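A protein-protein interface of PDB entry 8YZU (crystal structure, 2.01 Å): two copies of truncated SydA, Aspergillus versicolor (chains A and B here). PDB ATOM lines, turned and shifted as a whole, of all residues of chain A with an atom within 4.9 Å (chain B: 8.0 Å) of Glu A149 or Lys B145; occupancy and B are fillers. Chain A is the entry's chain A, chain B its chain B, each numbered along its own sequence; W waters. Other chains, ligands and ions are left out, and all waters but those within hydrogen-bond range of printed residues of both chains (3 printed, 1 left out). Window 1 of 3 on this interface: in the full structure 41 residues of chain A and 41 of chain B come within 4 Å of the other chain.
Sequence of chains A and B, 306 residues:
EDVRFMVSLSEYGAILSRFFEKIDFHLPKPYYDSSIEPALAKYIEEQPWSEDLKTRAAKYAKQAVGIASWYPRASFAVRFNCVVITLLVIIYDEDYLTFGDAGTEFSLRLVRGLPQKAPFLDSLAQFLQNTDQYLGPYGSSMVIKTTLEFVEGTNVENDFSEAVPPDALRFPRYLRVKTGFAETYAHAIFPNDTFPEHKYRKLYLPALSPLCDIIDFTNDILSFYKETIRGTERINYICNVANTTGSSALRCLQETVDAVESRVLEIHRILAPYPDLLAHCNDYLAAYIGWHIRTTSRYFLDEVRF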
ATOM      1  N   LYS A 145      -7.954   9.404  20.480  1.00  0.00           N
ATOM      2  CA  LYS A 145      -8.585  10.709  20.665  1.00  0.00           C
ATOM      3  C   LYS A 145      -7.719  11.625  21.528  1.00  0.00           C
ATOM      4  O   LYS A 145      -7.676  12.841  21.301  1.00  0.00           O
ATOM      5  CB  LYS A 145     -10.003  10.544  21.250  1.00  0.00           C
ATOM      6  CG  LYS A 145     -10.091  10.353  22.775  1.00  0.00           C
ATOM      7  CD  LYS A 145     -10.324  11.667  23.519  1.00  0.00           C
ATOM      8  CE  LYS A 145     -10.146  11.492  25.027  1.00  0.00           C
ATOM      9  NZ  LYS A 145     -10.173  12.789  25.755  1.00  0.00           N
ATOM     10  N   THR A 146      -7.035  11.059  22.529  1.00  0.00           N
ATOM     11  CA  THR A 146      -6.143  11.833  23.400  1.00  0.00           C
ATOM     12  C   THR A 146      -4.922  12.327  22.639  1.00  0.00           C
ATOM     13  O   THR A 146      -4.454  13.450  22.861  1.00  0.00           O
ATOM     14  CB  THR A 146      -5.701  10.968  24.589  1.00  0.00           C
ATOM     15  OG1 THR A 146      -6.850  10.562  25.338  1.00  0.00           O
ATOM     16  CG2 THR A 146      -4.725  11.707  25.500  1.00  0.00           C
ATOM     17  N   THR A 147      -4.376  11.493  21.747  1.00  0.00           N
ATOM     18  CA  THR A 147      -3.256  11.948  20.931  1.00  0.00           C
ATOM     19  C   THR A 147      -3.672  13.121  20.056  1.00  0.00           C
ATOM     20  O   THR A 147      -2.939  14.111  19.948  1.00  0.00           O
ATOM     21  CB  THR A 147      -2.718  10.792  20.081  1.00  0.00           C
ATOM     22  OG1 THR A 147      -2.344   9.719  20.953  1.00  0.00           O
ATOM     23  CG2 THR A 147      -1.491  11.226  19.280  1.00  0.00           C
ATOM     24  N   LEU A 148      -4.859  13.042  19.440  1.00  0.00           N
ATOM     25  CA  LEU A 148      -5.333  14.150  18.612  1.00  0.00           C
ATOM     26  C   LEU A 148      -5.412  15.438  19.418  1.00  0.00           C
ATOM     27  O   LEU A 148      -5.043  16.513  18.924  1.00  0.00           O
ATOM     28  CB  LEU A 148      -6.708  13.825  18.022  1.00  0.00           C
ATOM     29  CG  LEU A 148      -6.737  12.651  17.030  1.00  0.00           C
ATOM     30  CD1 LEU A 148      -8.160  12.423  16.556  1.00  0.00           C
ATOM     31  CD2 LEU A 148      -5.793  12.872  15.880  1.00  0.00           C
ATOM     32  N   GLU A 149      -5.924  15.339  20.650  1.00  0.00           N
ATOM     33  CA  GLU A 149      -5.994  16.489  21.552  1.00  0.00           C
ATOM     34  C   GLU A 149      -4.607  17.008  21.893  1.00  0.00           C
ATOM     35  O   GLU A 149      -4.380  18.224  21.905  1.00  0.00           O
ATOM     36  CB  GLU A 149      -6.746  16.106  22.836  1.00  0.00           C
ATOM     37  CG  GLU A 149      -8.239  15.995  22.673  1.00  0.00           C
ATOM     38  CD  GLU A 149      -8.957  15.487  23.930  1.00  0.00           C
ATOM     39  OE1 GLU A 149      -8.467  14.550  24.623  1.00  0.00           O
ATOM     40  OE2 GLU A 149     -10.017  16.065  24.236  1.00  0.00           O
ATOM     41  N   PHE A 150      -3.670  16.097  22.188  1.00  0.00           N
ATOM     42  CA  PHE A 150      -2.334  16.507  22.588  1.00  0.00           C
ATOM     43  C   PHE A 150      -1.617  17.252  21.473  1.00  0.00           C
ATOM     44  O   PHE A 150      -0.934  18.247  21.732  1.00  0.00           O
ATOM     45  CB  PHE A 150      -1.502  15.299  23.027  1.00  0.00           C
ATOM     46  CG  PHE A 150      -0.026  15.596  23.131  1.00  0.00           C
ATOM     47  CD1 PHE A 150       0.487  16.235  24.248  1.00  0.00           C
ATOM     48  CD2 PHE A 150       0.857  15.240  22.104  1.00  0.00           C
ATOM     49  CE1 PHE A 150       1.839  16.527  24.354  1.00  0.00           C
ATOM     50  CE2 PHE A 150       2.214  15.543  22.204  1.00  0.00           C
ATOM     51  CZ  PHE A 150       2.709  16.170  23.338  1.00  0.00           C
ATOM     52  N   VAL A 151      -1.723  16.772  20.233  1.00  0.00           N
ATOM     53  CA  VAL A 151      -1.064  17.471  19.134  1.00  0.00           C
ATOM     54  C   VAL A 151      -1.604  18.892  19.023  1.00  0.00           C
ATOM     55  O   VAL A 151      -0.842  19.855  18.875  1.00  0.00           O
ATOM     56  CB  VAL A 151      -1.238  16.704  17.807  1.00  0.00           C
ATOM     57  CG1 VAL A 151      -0.688  17.554  16.645  1.00  0.00           C
ATOM     58  CG2 VAL A 151      -0.531  15.350  17.859  1.00  0.00           C
ATOM     59  N   GLU A 152      -2.931  19.045  19.093  1.00  0.00           N
ATOM     60  CA  GLU A 152      -3.507  20.370  18.891  1.00  0.00           C
ATOM     61  C   GLU A 152      -3.322  21.257  20.119  1.00  0.00           C
ATOM     62  O   GLU A 152      -3.090  22.461  19.978  1.00  0.00           O
ATOM     63  CB  GLU A 152      -4.985  20.259  18.507  1.00  0.00           C
ATOM     64  CG  GLU A 152      -5.225  20.131  16.962  1.00  0.00           C
ATOM     65  CD  GLU A 152      -4.403  21.121  16.166  1.00  0.00           C
ATOM     66  OE1 GLU A 152      -4.741  22.325  16.144  1.00  0.00           O
ATOM     67  OE2 GLU A 152      -3.397  20.702  15.554  1.00  0.00           O
ATOM     68  N   GLY A 153      -3.409  20.686  21.324  1.00  0.00           N
ATOM     69  CA  GLY A 153      -3.146  21.473  22.516  1.00  0.00           C
ATOM     70  C   GLY A 153      -1.736  22.038  22.544  1.00  0.00           C
ATOM     71  O   GLY A 153      -1.525  23.191  22.936  1.00  0.00           O
ATOM     72  N   THR A 154      -0.753  21.228  22.159  1.00  0.00           N
ATOM     73  CA  THR A 154       0.635  21.693  22.079  1.00  0.00           C
ATOM     74  C   THR A 154       0.791  22.789  21.027  1.00  0.00           C
ATOM     75  O   THR A 154       1.567  23.734  21.214  1.00  0.00           O
ATOM     76  CB  THR A 154       1.557  20.501  21.768  1.00  0.00           C
ATOM     77  OG1 THR A 154       1.439  19.520  22.808  1.00  0.00           O
ATOM     78  CG2 THR A 154       3.063  20.933  21.589  1.00  0.00           C
ATOM     79  N   VAL A 177      -6.760  19.305  29.898  1.00  0.00           N
ATOM     80  CA  VAL A 177      -7.167  18.015  29.336  1.00  0.00           C
ATOM     81  C   VAL A 177      -6.474  17.807  27.999  1.00  0.00           C
ATOM     82  O   VAL A 177      -5.808  16.785  27.782  1.00  0.00           O
ATOM     83  CB  VAL A 177      -8.695  17.911  29.202  1.00  0.00           C
ATOM     84  CG1 VAL A 177      -9.088  16.656  28.354  1.00  0.00           C
ATOM     85  CG2 VAL A 177      -9.349  17.863  30.574  1.00  0.00           C
ATOM     86  N   LYS A 178      -6.521  18.833  27.136  1.00  0.00           N
ATOM     87  CA  LYS A 178      -5.883  18.778  25.819  1.00  0.00           C
ATOM     88  C   LYS A 178      -4.383  18.505  25.907  1.00  0.00           C
ATOM     89  O   LYS A 178      -3.871  17.620  25.210  1.00  0.00           O
ATOM     90  CB  LYS A 178      -6.121  20.084  25.048  1.00  0.00           C
ATOM     91  CG  LYS A 178      -7.596  20.457  24.854  1.00  0.00           C
ATOM     92  CD  LYS A 178      -8.360  19.426  24.041  1.00  0.00           C
ATOM     93  CE  LYS A 178      -9.794  19.892  23.765  1.00  0.00           C
ATOM     94  NZ  LYS A 178     -10.841  18.939  24.276  1.00  0.00           N
ATOM     95  N   GLU A 183      -5.256  10.250  29.538  1.00  0.00           N
ATOM     96  CA  GLU A 183      -5.996   9.005  29.315  1.00  0.00           C
ATOM     97  C   GLU A 183      -5.121   7.910  28.722  1.00  0.00           C
ATOM     98  O   GLU A 183      -5.327   6.728  29.030  1.00  0.00           O
ATOM     99  CB  GLU A 183      -7.238   9.254  28.434  1.00  0.00           C
ATOM    100  CG  GLU A 183      -8.422   9.799  29.253  1.00  0.00           C
ATOM    101  CD  GLU A 183      -9.546  10.378  28.419  1.00  0.00           C
ATOM    102  OE1 GLU A 183      -9.447  11.597  28.104  1.00  0.00           O
ATOM    103  OE2 GLU A 183     -10.523   9.642  28.119  1.00  0.00           O
ATOM    104  N   LEU B 110     -10.603   3.373  11.309  1.00  0.00           N
ATOM    105  CA  LEU B 110     -10.488   4.765  10.882  1.00  0.00           C
ATOM    106  C   LEU B 110      -9.023   5.196  10.772  1.00  0.00           C
ATOM    107  O   LEU B 110      -8.586   5.691   9.726  1.00  0.00           O
ATOM    108  CB  LEU B 110     -11.240   5.669  11.861  1.00  0.00           C
ATOM    109  CG  LEU B 110     -11.367   7.141  11.453  1.00  0.00           C
ATOM    110  CD1 LEU B 110     -12.264   7.252  10.233  1.00  0.00           C
ATOM    111  CD2 LEU B 110     -11.909   7.995  12.608  1.00  0.00           C
ATOM    112  N   LEU B 128     -15.984  12.772   8.873  1.00  0.00           N
ATOM    113  CA  LEU B 128     -14.787  13.170   9.606  1.00  0.00           C
ATOM    114  C   LEU B 128     -13.668  13.591   8.664  1.00  0.00           C
ATOM    115  O   LEU B 128     -12.850  14.446   9.017  1.00  0.00           O
ATOM    116  CB  LEU B 128     -14.314  12.020  10.500  1.00  0.00           C
ATOM    117  CG  LEU B 128     -15.216  11.626  11.674  1.00  0.00           C
ATOM    118  CD1 LEU B 128     -14.593  10.497  12.477  1.00  0.00           C
ATOM    119  CD2 LEU B 128     -15.500  12.840  12.565  1.00  0.00           C
ATOM    120  N   TYR B 138      -7.852  22.861  14.280  1.00  0.00           N
ATOM    121  CA  TYR B 138      -8.218  22.511  15.653  1.00  0.00           C
ATOM    122  C   TYR B 138      -9.643  21.972  15.709  1.00  0.00           C
ATOM    123  O   TYR B 138      -9.902  20.938  16.338  1.00  0.00           O
ATOM    124  CB  TYR B 138      -8.057  23.730  16.562  1.00  0.00           C
ATOM    125  CG  TYR B 138      -8.200  23.460  18.039  1.00  0.00           C
ATOM    126  CD1 TYR B 138      -9.462  23.361  18.624  1.00  0.00           C
ATOM    127  CD2 TYR B 138      -7.088  23.342  18.861  1.00  0.00           C
ATOM    128  CE1 TYR B 138      -9.615  23.141  19.977  1.00  0.00           C
ATOM    129  CE2 TYR B 138      -7.226  23.115  20.227  1.00  0.00           C
ATOM    130  CZ  TYR B 138      -8.501  23.018  20.775  1.00  0.00           C
ATOM    131  OH  TYR B 138      -8.671  22.793  22.123  1.00  0.00           O
ATOM    132  N   GLY B 139     -10.570  22.636  15.019  1.00  0.00           N
ATOM    133  CA  GLY B 139     -11.946  22.151  14.987  1.00  0.00           C
ATOM    134  C   GLY B 139     -12.070  20.770  14.366  1.00  0.00           C
ATOM    135  O   GLY B 139     -12.779  19.905  14.892  1.00  0.00           O
ATOM    136  N   SER B 140     -11.357  20.532  13.257  1.00  0.00           N
ATOM    137  CA  SER B 140     -11.389  19.215  12.622  1.00  0.00           C
ATOM    138  C   SER B 140     -10.871  18.115  13.548  1.00  0.00           C
ATOM    139  O   SER B 140     -11.445  17.021  13.596  1.00  0.00           O
ATOM    140  CB  SER B 140     -10.583  19.246  11.323  1.00  0.00           C
ATOM    141  OG  SER B 140     -11.286  19.975  10.339  1.00  0.00           O
ATOM    142  N   SER B 141      -9.784  18.369  14.280  1.00  0.00           N
ATOM    143  CA  SER B 141      -9.299  17.369  15.242  1.00  0.00           C
ATOM    144  C   SER B 141     -10.339  17.097  16.327  1.00  0.00           C
ATOM    145  O   SER B 141     -10.539  15.949  16.740  1.00  0.00           O
ATOM    146  CB  SER B 141      -7.995  17.828  15.893  1.00  0.00           C
ATOM    147  OG  SER B 141      -6.959  18.083  14.933  1.00  0.00           O
ATOM    148  N   MET B 142     -10.980  18.153  16.827  1.00  0.00           N
ATOM    149  CA  MET B 142     -11.960  18.015  17.902  1.00  0.00           C
ATOM    150  C   MET B 142     -13.182  17.225  17.435  1.00  0.00           C
ATOM    151  O   MET B 142     -13.727  16.420  18.198  1.00  0.00           O
ATOM    152  CB  MET B 142     -12.344  19.409  18.394  1.00  0.00           C
ATOM    153  CG  MET B 142     -11.168  20.129  19.120  1.00  0.00           C
ATOM    154  SD  MET B 142     -10.190  18.995  20.170  1.00  0.00           S
ATOM    155  CE  MET B 142      -8.507  19.305  19.641  1.00  0.00           C
ATOM    156  N   VAL B 143     -13.623  17.424  16.184  1.00  0.00           N
ATOM    157  CA  VAL B 143     -14.771  16.645  15.700  1.00  0.00           C
ATOM    158  C   VAL B 143     -14.412  15.167  15.606  1.00  0.00           C
ATOM    159  O   VAL B 143     -15.220  14.290  15.929  1.00  0.00           O
ATOM    160  CB  VAL B 143     -15.279  17.189  14.352  1.00  0.00           C
ATOM    161  CG1 VAL B 143     -16.404  16.311  13.798  1.00  0.00           C
ATOM    162  CG2 VAL B 143     -15.787  18.590  14.530  1.00  0.00           C
ATOM    163  N   ILE B 144     -13.202  14.863  15.152  1.00  0.00           N
ATOM    164  CA  ILE B 144     -12.781  13.467  15.077  1.00  0.00           C
ATOM    165  C   ILE B 144     -12.722  12.857  16.474  1.00  0.00           C
ATOM    166  O   ILE B 144     -13.309  11.795  16.727  1.00  0.00           O
ATOM    167  CB  ILE B 144     -11.421  13.348  14.358  1.00  0.00           C
ATOM    168  CG1 ILE B 144     -11.568  13.634  12.858  1.00  0.00           C
ATOM    169  CG2 ILE B 144     -10.876  11.957  14.543  1.00  0.00           C
ATOM    170  CD1 ILE B 144     -10.244  14.074  12.188  1.00  0.00           C
ATOM    171  N   LYS B 145     -12.013  13.513  17.407  1.00  0.00           N
ATOM    172  CA  LYS B 145     -11.848  12.897  18.723  1.00  0.00           C
ATOM    173  C   LYS B 145     -13.183  12.801  19.459  1.00  0.00           C
ATOM    174  O   LYS B 145     -13.405  11.856  20.224  1.00  0.00           O
ATOM    175  CB  LYS B 145     -10.811  13.652  19.562  1.00  0.00           C
ATOM    176  CG  LYS B 145     -11.271  15.009  20.158  1.00  0.00           C
ATOM    177  CD  LYS B 145     -11.687  14.856  21.617  1.00  0.00           C
ATOM    178  CE  LYS B 145     -12.636  15.957  22.078  1.00  0.00           C
ATOM    179  NZ  LYS B 145     -12.993  15.741  23.552  1.00  0.00           N
ATOM    180  N   THR B 146     -14.068  13.787  19.270  1.00  0.00           N
ATOM    181  CA  THR B 146     -15.400  13.727  19.881  1.00  0.00           C
ATOM    182  C   THR B 146     -16.222  12.580  19.300  1.00  0.00           C
ATOM    183  O   THR B 146     -16.956  11.891  20.021  1.00  0.00           O
ATOM    184  CB  THR B 146     -16.124  15.056  19.656  1.00  0.00           C
ATOM    185  OG1 THR B 146     -15.358  16.119  20.237  1.00  0.00           O
ATOM    186  CG2 THR B 146     -17.526  15.030  20.251  1.00  0.00           C
ATOM    187  N   THR B 147     -16.110  12.352  17.997  1.00  0.00           N
ATOM    188  CA  THR B 147     -16.831  11.240  17.384  1.00  0.00           C
ATOM    189  C   THR B 147     -16.382   9.897  17.957  1.00  0.00           C
ATOM    190  O   THR B 147     -17.219   9.035  18.252  1.00  0.00           O
ATOM    191  CB  THR B 147     -16.634  11.288  15.873  1.00  0.00           C
ATOM    192  OG1 THR B 147     -17.189  12.520  15.394  1.00  0.00           O
ATOM    193  CG2 THR B 147     -17.319  10.091  15.184  1.00  0.00           C
ATOM    194  N   LEU B 148     -15.071   9.699  18.133  1.00  0.00           N
ATOM    195  CA  LEU B 148     -14.588   8.454  18.733  1.00  0.00           C
ATOM    196  C   LEU B 148     -15.127   8.291  20.148  1.00  0.00           C
ATOM    197  O   LEU B 148     -15.488   7.186  20.565  1.00  0.00           O
ATOM    198  CB  LEU B 148     -13.053   8.431  18.754  1.00  0.00           C
ATOM    199  CG  LEU B 148     -12.319   8.714  17.437  1.00  0.00           C
ATOM    200  CD1 LEU B 148     -10.808   8.681  17.642  1.00  0.00           C
ATOM    201  CD2 LEU B 148     -12.750   7.762  16.338  1.00  0.00           C
ATOM    202  N   GLU B 149     -15.162   9.381  20.912  1.00  0.00           N
ATOM    203  CA  GLU B 149     -15.700   9.316  22.266  1.00  0.00           C
ATOM    204  C   GLU B 149     -17.182   8.935  22.244  1.00  0.00           C
ATOM    205  O   GLU B 149     -17.629   8.063  23.005  1.00  0.00           O
ATOM    206  CB  GLU B 149     -15.473  10.667  22.958  1.00  0.00           C
ATOM    207  CG  GLU B 149     -14.073  10.804  23.530  1.00  0.00           C
ATOM    208  CD  GLU B 149     -13.827  12.148  24.221  1.00  0.00           C
ATOM    209  OE1 GLU B 149     -13.184  12.131  25.296  1.00  0.00           O
ATOM    210  OE2 GLU B 149     -14.285  13.206  23.708  1.00  0.00           O
ATOM    211  N   PHE B 150     -17.954   9.558  21.346  1.00  0.00           N
ATOM    212  CA  PHE B 150     -19.385   9.301  21.284  1.00  0.00           C
ATOM    213  C   PHE B 150     -19.671   7.865  20.877  1.00  0.00           C
ATOM    214  O   PHE B 150     -20.570   7.221  21.437  1.00  0.00           O
ATOM    215  CB  PHE B 150     -20.056  10.269  20.309  1.00  0.00           C
ATOM    216  CG  PHE B 150     -21.421   9.813  19.845  1.00  0.00           C
ATOM    217  CD1 PHE B 150     -22.537   9.973  20.673  1.00  0.00           C
ATOM    218  CD2 PHE B 150     -21.594   9.215  18.598  1.00  0.00           C
ATOM    219  CE1 PHE B 150     -23.792   9.545  20.269  1.00  0.00           C
ATOM    220  CE2 PHE B 150     -22.866   8.776  18.179  1.00  0.00           C
ATOM    221  CZ  PHE B 150     -23.962   8.952  19.006  1.00  0.00           C
ATOM    222  N   VAL B 151     -18.940   7.348  19.885  1.00  0.00           N
ATOM    223  CA  VAL B 151     -19.187   5.981  19.439  1.00  0.00           C
ATOM    224  C   VAL B 151     -18.943   5.016  20.590  1.00  0.00           C
ATOM    225  O   VAL B 151     -19.769   4.135  20.871  1.00  0.00           O
ATOM    226  CB  VAL B 151     -18.315   5.650  18.214  1.00  0.00           C
ATOM    227  CG1 VAL B 151     -18.371   4.152  17.879  1.00  0.00           C
ATOM    228  CG2 VAL B 151     -18.756   6.477  17.004  1.00  0.00           C
ATOM    229  N   VAL B 177     -19.279  13.600  29.110  1.00  0.00           N
ATOM    230  CA  VAL B 177     -18.377  14.123  28.084  1.00  0.00           C
ATOM    231  C   VAL B 177     -18.338  13.156  26.905  1.00  0.00           C
ATOM    232  O   VAL B 177     -18.478  13.554  25.742  1.00  0.00           O
ATOM    233  CB  VAL B 177     -16.974  14.381  28.664  1.00  0.00           C
ATOM    234  CG1 VAL B 177     -15.955  14.537  27.544  1.00  0.00           C
ATOM    235  CG2 VAL B 177     -16.973  15.638  29.529  1.00  0.00           C
ATOM    236  N   LYS B 178     -18.210  11.865  27.201  1.00  0.00           N
ATOM    237  CA  LYS B 178     -18.095  10.855  26.152  1.00  0.00           C
ATOM    238  C   LYS B 178     -19.368  10.760  25.320  1.00  0.00           C
ATOM    239  O   LYS B 178     -19.313  10.691  24.085  1.00  0.00           O
ATOM    240  CB  LYS B 178     -17.777   9.501  26.786  1.00  0.00           C
ATOM    241  CG  LYS B 178     -16.512   9.506  27.657  1.00  0.00           C
ATOM    242  CD  LYS B 178     -15.270   9.699  26.785  1.00  0.00           C
ATOM    243  CE  LYS B 178     -13.968   9.564  27.577  1.00  0.00           C
ATOM    244  NZ  LYS B 178     -13.063  10.758  27.364  1.00  0.00           N
ATOM    245  N   PHE B 181     -21.253  14.324  22.740  1.00  0.00           N
ATOM    246  CA  PHE B 181     -20.916  14.810  21.405  1.00  0.00           C
ATOM    247  C   PHE B 181     -20.825  16.332  21.361  1.00  0.00           C
ATOM    248  O   PHE B 181     -20.966  16.924  20.292  1.00  0.00           O
ATOM    249  CB  PHE B 181     -21.946  14.293  20.375  1.00  0.00           C
ATOM    250  CG  PHE B 181     -21.469  14.305  18.940  1.00  0.00           C
ATOM    251  CD1 PHE B 181     -20.386  13.539  18.540  1.00  0.00           C
ATOM    252  CD2 PHE B 181     -22.133  15.066  17.989  1.00  0.00           C
ATOM    253  CE1 PHE B 181     -19.961  13.540  17.221  1.00  0.00           C
ATOM    254  CE2 PHE B 181     -21.710  15.072  16.667  1.00  0.00           C
ATOM    255  CZ  PHE B 181     -20.616  14.317  16.284  1.00  0.00           C
ATOM    256  N   ALA B 182     -20.605  16.993  22.513  1.00  0.00           N
ATOM    257  CA  ALA B 182     -20.829  18.441  22.602  1.00  0.00           C
ATOM    258  C   ALA B 182     -19.845  19.241  21.752  1.00  0.00           C
ATOM    259  O   ALA B 182     -20.224  20.256  21.146  1.00  0.00           O
ATOM    260  CB  ALA B 182     -20.747  18.908  24.058  1.00  0.00           C
ATOM    261  N   GLU B 183     -18.569  18.845  21.737  1.00  0.00           N
ATOM    262  CA  GLU B 183     -17.569  19.689  21.088  1.00  0.00           C
ATOM    263  C   GLU B 183     -17.840  19.836  19.599  1.00  0.00           C
ATOM    264  O   GLU B 183     -17.508  20.869  19.000  1.00  0.00           O
ATOM    265  CB  GLU B 183     -16.163  19.128  21.330  1.00  0.00           C
ATOM    266  CG  GLU B 183     -15.508  19.701  22.591  1.00  0.00           C
ATOM    267  CD  GLU B 183     -14.279  18.943  23.036  1.00  0.00           C
ATOM    268  OE1 GLU B 183     -14.424  17.890  23.704  1.00  0.00           O
ATOM    269  OE2 GLU B 183     -13.164  19.429  22.751  1.00  0.00           O
ATOM    270  N   THR B 184     -18.449  18.825  18.978  1.00  0.00           N
ATOM    271  CA  THR B 184     -18.694  18.931  17.542  1.00  0.00           C
ATOM    272  C   THR B 184     -19.669  20.061  17.256  1.00  0.00           C
ATOM    273  O   THR B 184     -19.462  20.839  16.316  1.00  0.00           O
ATOM    274  CB  THR B 184     -19.211  17.599  16.987  1.00  0.00           C
ATOM    275  OG1 THR B 184     -18.212  16.580  17.135  1.00  0.00           O
ATOM    276  CG2 THR B 184     -19.620  17.725  15.533  1.00  0.00           C
ATOM    277  N   HIS B 187     -17.970  23.702  18.217  1.00  0.00           N
ATOM    278  CA  HIS B 187     -17.035  24.259  17.252  1.00  0.00           C
ATOM    279  C   HIS B 187     -17.752  24.932  16.098  1.00  0.00           C
ATOM    280  O   HIS B 187     -17.258  25.934  15.570  1.00  0.00           O
ATOM    281  CB  HIS B 187     -16.061  23.178  16.785  1.00  0.00           C
ATOM    282  CG  HIS B 187     -14.879  23.061  17.691  1.00  0.00           C
ATOM    283  ND1 HIS B 187     -13.833  23.960  17.654  1.00  0.00           N
ATOM    284  CD2 HIS B 187     -14.624  22.227  18.728  1.00  0.00           C
ATOM    285  CE1 HIS B 187     -12.956  23.649  18.593  1.00  0.00           C
ATOM    286  NE2 HIS B 187     -13.411  22.605  19.262  1.00  0.00           N
ATOM    287  N   CYS B 212     -19.736  23.644  26.086  1.00  0.00           N
ATOM    288  CA  CYS B 212     -19.948  22.202  26.027  1.00  0.00           C
ATOM    289  C   CYS B 212     -20.783  21.733  27.210  1.00  0.00           C
ATOM    290  O   CYS B 212     -21.663  20.875  27.057  1.00  0.00           O
ATOM    291  CB  CYS B 212     -18.598  21.500  26.009  1.00  0.00           C
ATOM    292  SG  CYS B 212     -17.861  21.535  24.368  1.00  0.00           S
HETATM  293  O   HOH W   1      -4.691  16.587  16.015  1.00  0.00           O
HETATM  294  O   HOH W   2      -3.931  17.931  13.865  1.00  0.00           O
HETATM  295  O   HOH W   3     -12.135  15.058  26.652  1.00  0.00           O
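Glu A149 touches just one residue of chain B: Lys B145. Val A177 touches none of the printed residues of chain B. Of the printed residues of chain A, Ser B141 touches Glu A152. Val B143 touches none of the printed residues of chain A. Of the printed residues of chain A, Ile B144 touches Leu A148 (3.4 Å). Lys B145 touches three residues of chain A. The nearest residue of chain B that does not touch Glu A149 is Met B142 (4.2 Å).
Among the printed residues, pairs that only touch across the chains: Lys A145 with Lys B145 (3.6 Å), Lys A145 with Lys B178 (3.8 Å), Leu A148 with Ile B144 (3.4 Å), Glu A152 with Tyr B138 (3.5 Å), Glu A152 with Ser B141 (3.4 Å), Glu A152 with Met B142 (3.8 Å), Lys A178 with Tyr B138 (3.5 Å), Lys A178 with Met B142 (3.7 Å) and Lys A178 with Lys B145 (3.9 Å).
Of the 24 printed residues of chain B, 8 touch a printed residue of chain A. Printed residues of chain B that touch a printed residue of chain A: Tyr B138, Ser B141, Met B142, Ile B144, Lys B145, Glu B149, Lys B178 and Glu B183. Hydrophobic or aromatic side chains of chain B within 4 Å of the printed part of chain A: Tyr B138, Met B142 and Ile B144. Of the 13 printed residues of chain A, 6 touch a printed residue of chain B. Hydrophobic or aromatic side chains of chain A that line the printed part of chain B: Leu A148.
Water W1 lies within hydrogen-bond range of OG of Ser B141 (2.9 Å) and O of Leu A148 (2.9 Å). Water W3 lies within hydrogen-bond range of NZ of Lys A145, NZ of Lys B145, OE2 of Glu A149 and OE1 of Glu B149. Water W2 bridges the side-chain hydroxyl (OG) of Ser B141 (3.2 Å) and the side-chain carboxylate (OE2) of Glu A152 (3.3 Å).
Lys B145 touches its own counterpart, Lys A145. Lys A145 touches Glu B149, and with the chains exchanged Glu A149 touches Lys B145. Lys A145 touches Lys B178, and with the chains exchanged Lys A178 touches Lys B145. Lys A178 touches Glu B183, and with the chains exchanged Glu A183 touches Lys B178. Positions printed for both chains: 145, 146, 147, 148, 149, 150, 151, 177, 178 and 183.
The side-chain amino group of Lys A145 lies within salt-bridge range of the side-chain carboxylate of Glu A149, 2.7 Å away. NZ of Lys A145 is in salt-bridge range of OE1 of Glu A183, 2.7 Å away. O of Lys A178 sits close to N of Phe A150, 3.4 Å away. The side-chain amino group (NZ) of Lys B145 is in salt-bridge range of the side-chain carboxylate (OE2) of Glu B149, at 2.8 Å. The side-chain carboxylate of Glu B183 is in salt-bridge range of the side-chain amino group of Lys B145. The backbone NH (N) of Phe B150 sits close to the backbone carbonyl oxygen (O) of Lys B178 (3.3 Å).
The side-chain carboxylate (OE1) of Glu B149 lies within salt-bridge range of the side-chain amino group (NZ) of Lys A145, at 3.1 Å. The side-chain carboxylate (OE2) of Glu A149 is in salt-bridge range of the side-chain amino group (NZ) of Lys B145 (3.1 Å). NZ of Lys A178 lies within salt-bridge range of OE2 of Glu B183, 2.8 Å away. The side-chain carboxylate of Glu A183 lies within salt-bridge range of the side-chain amino group of Lys B178 (2.9 Å).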
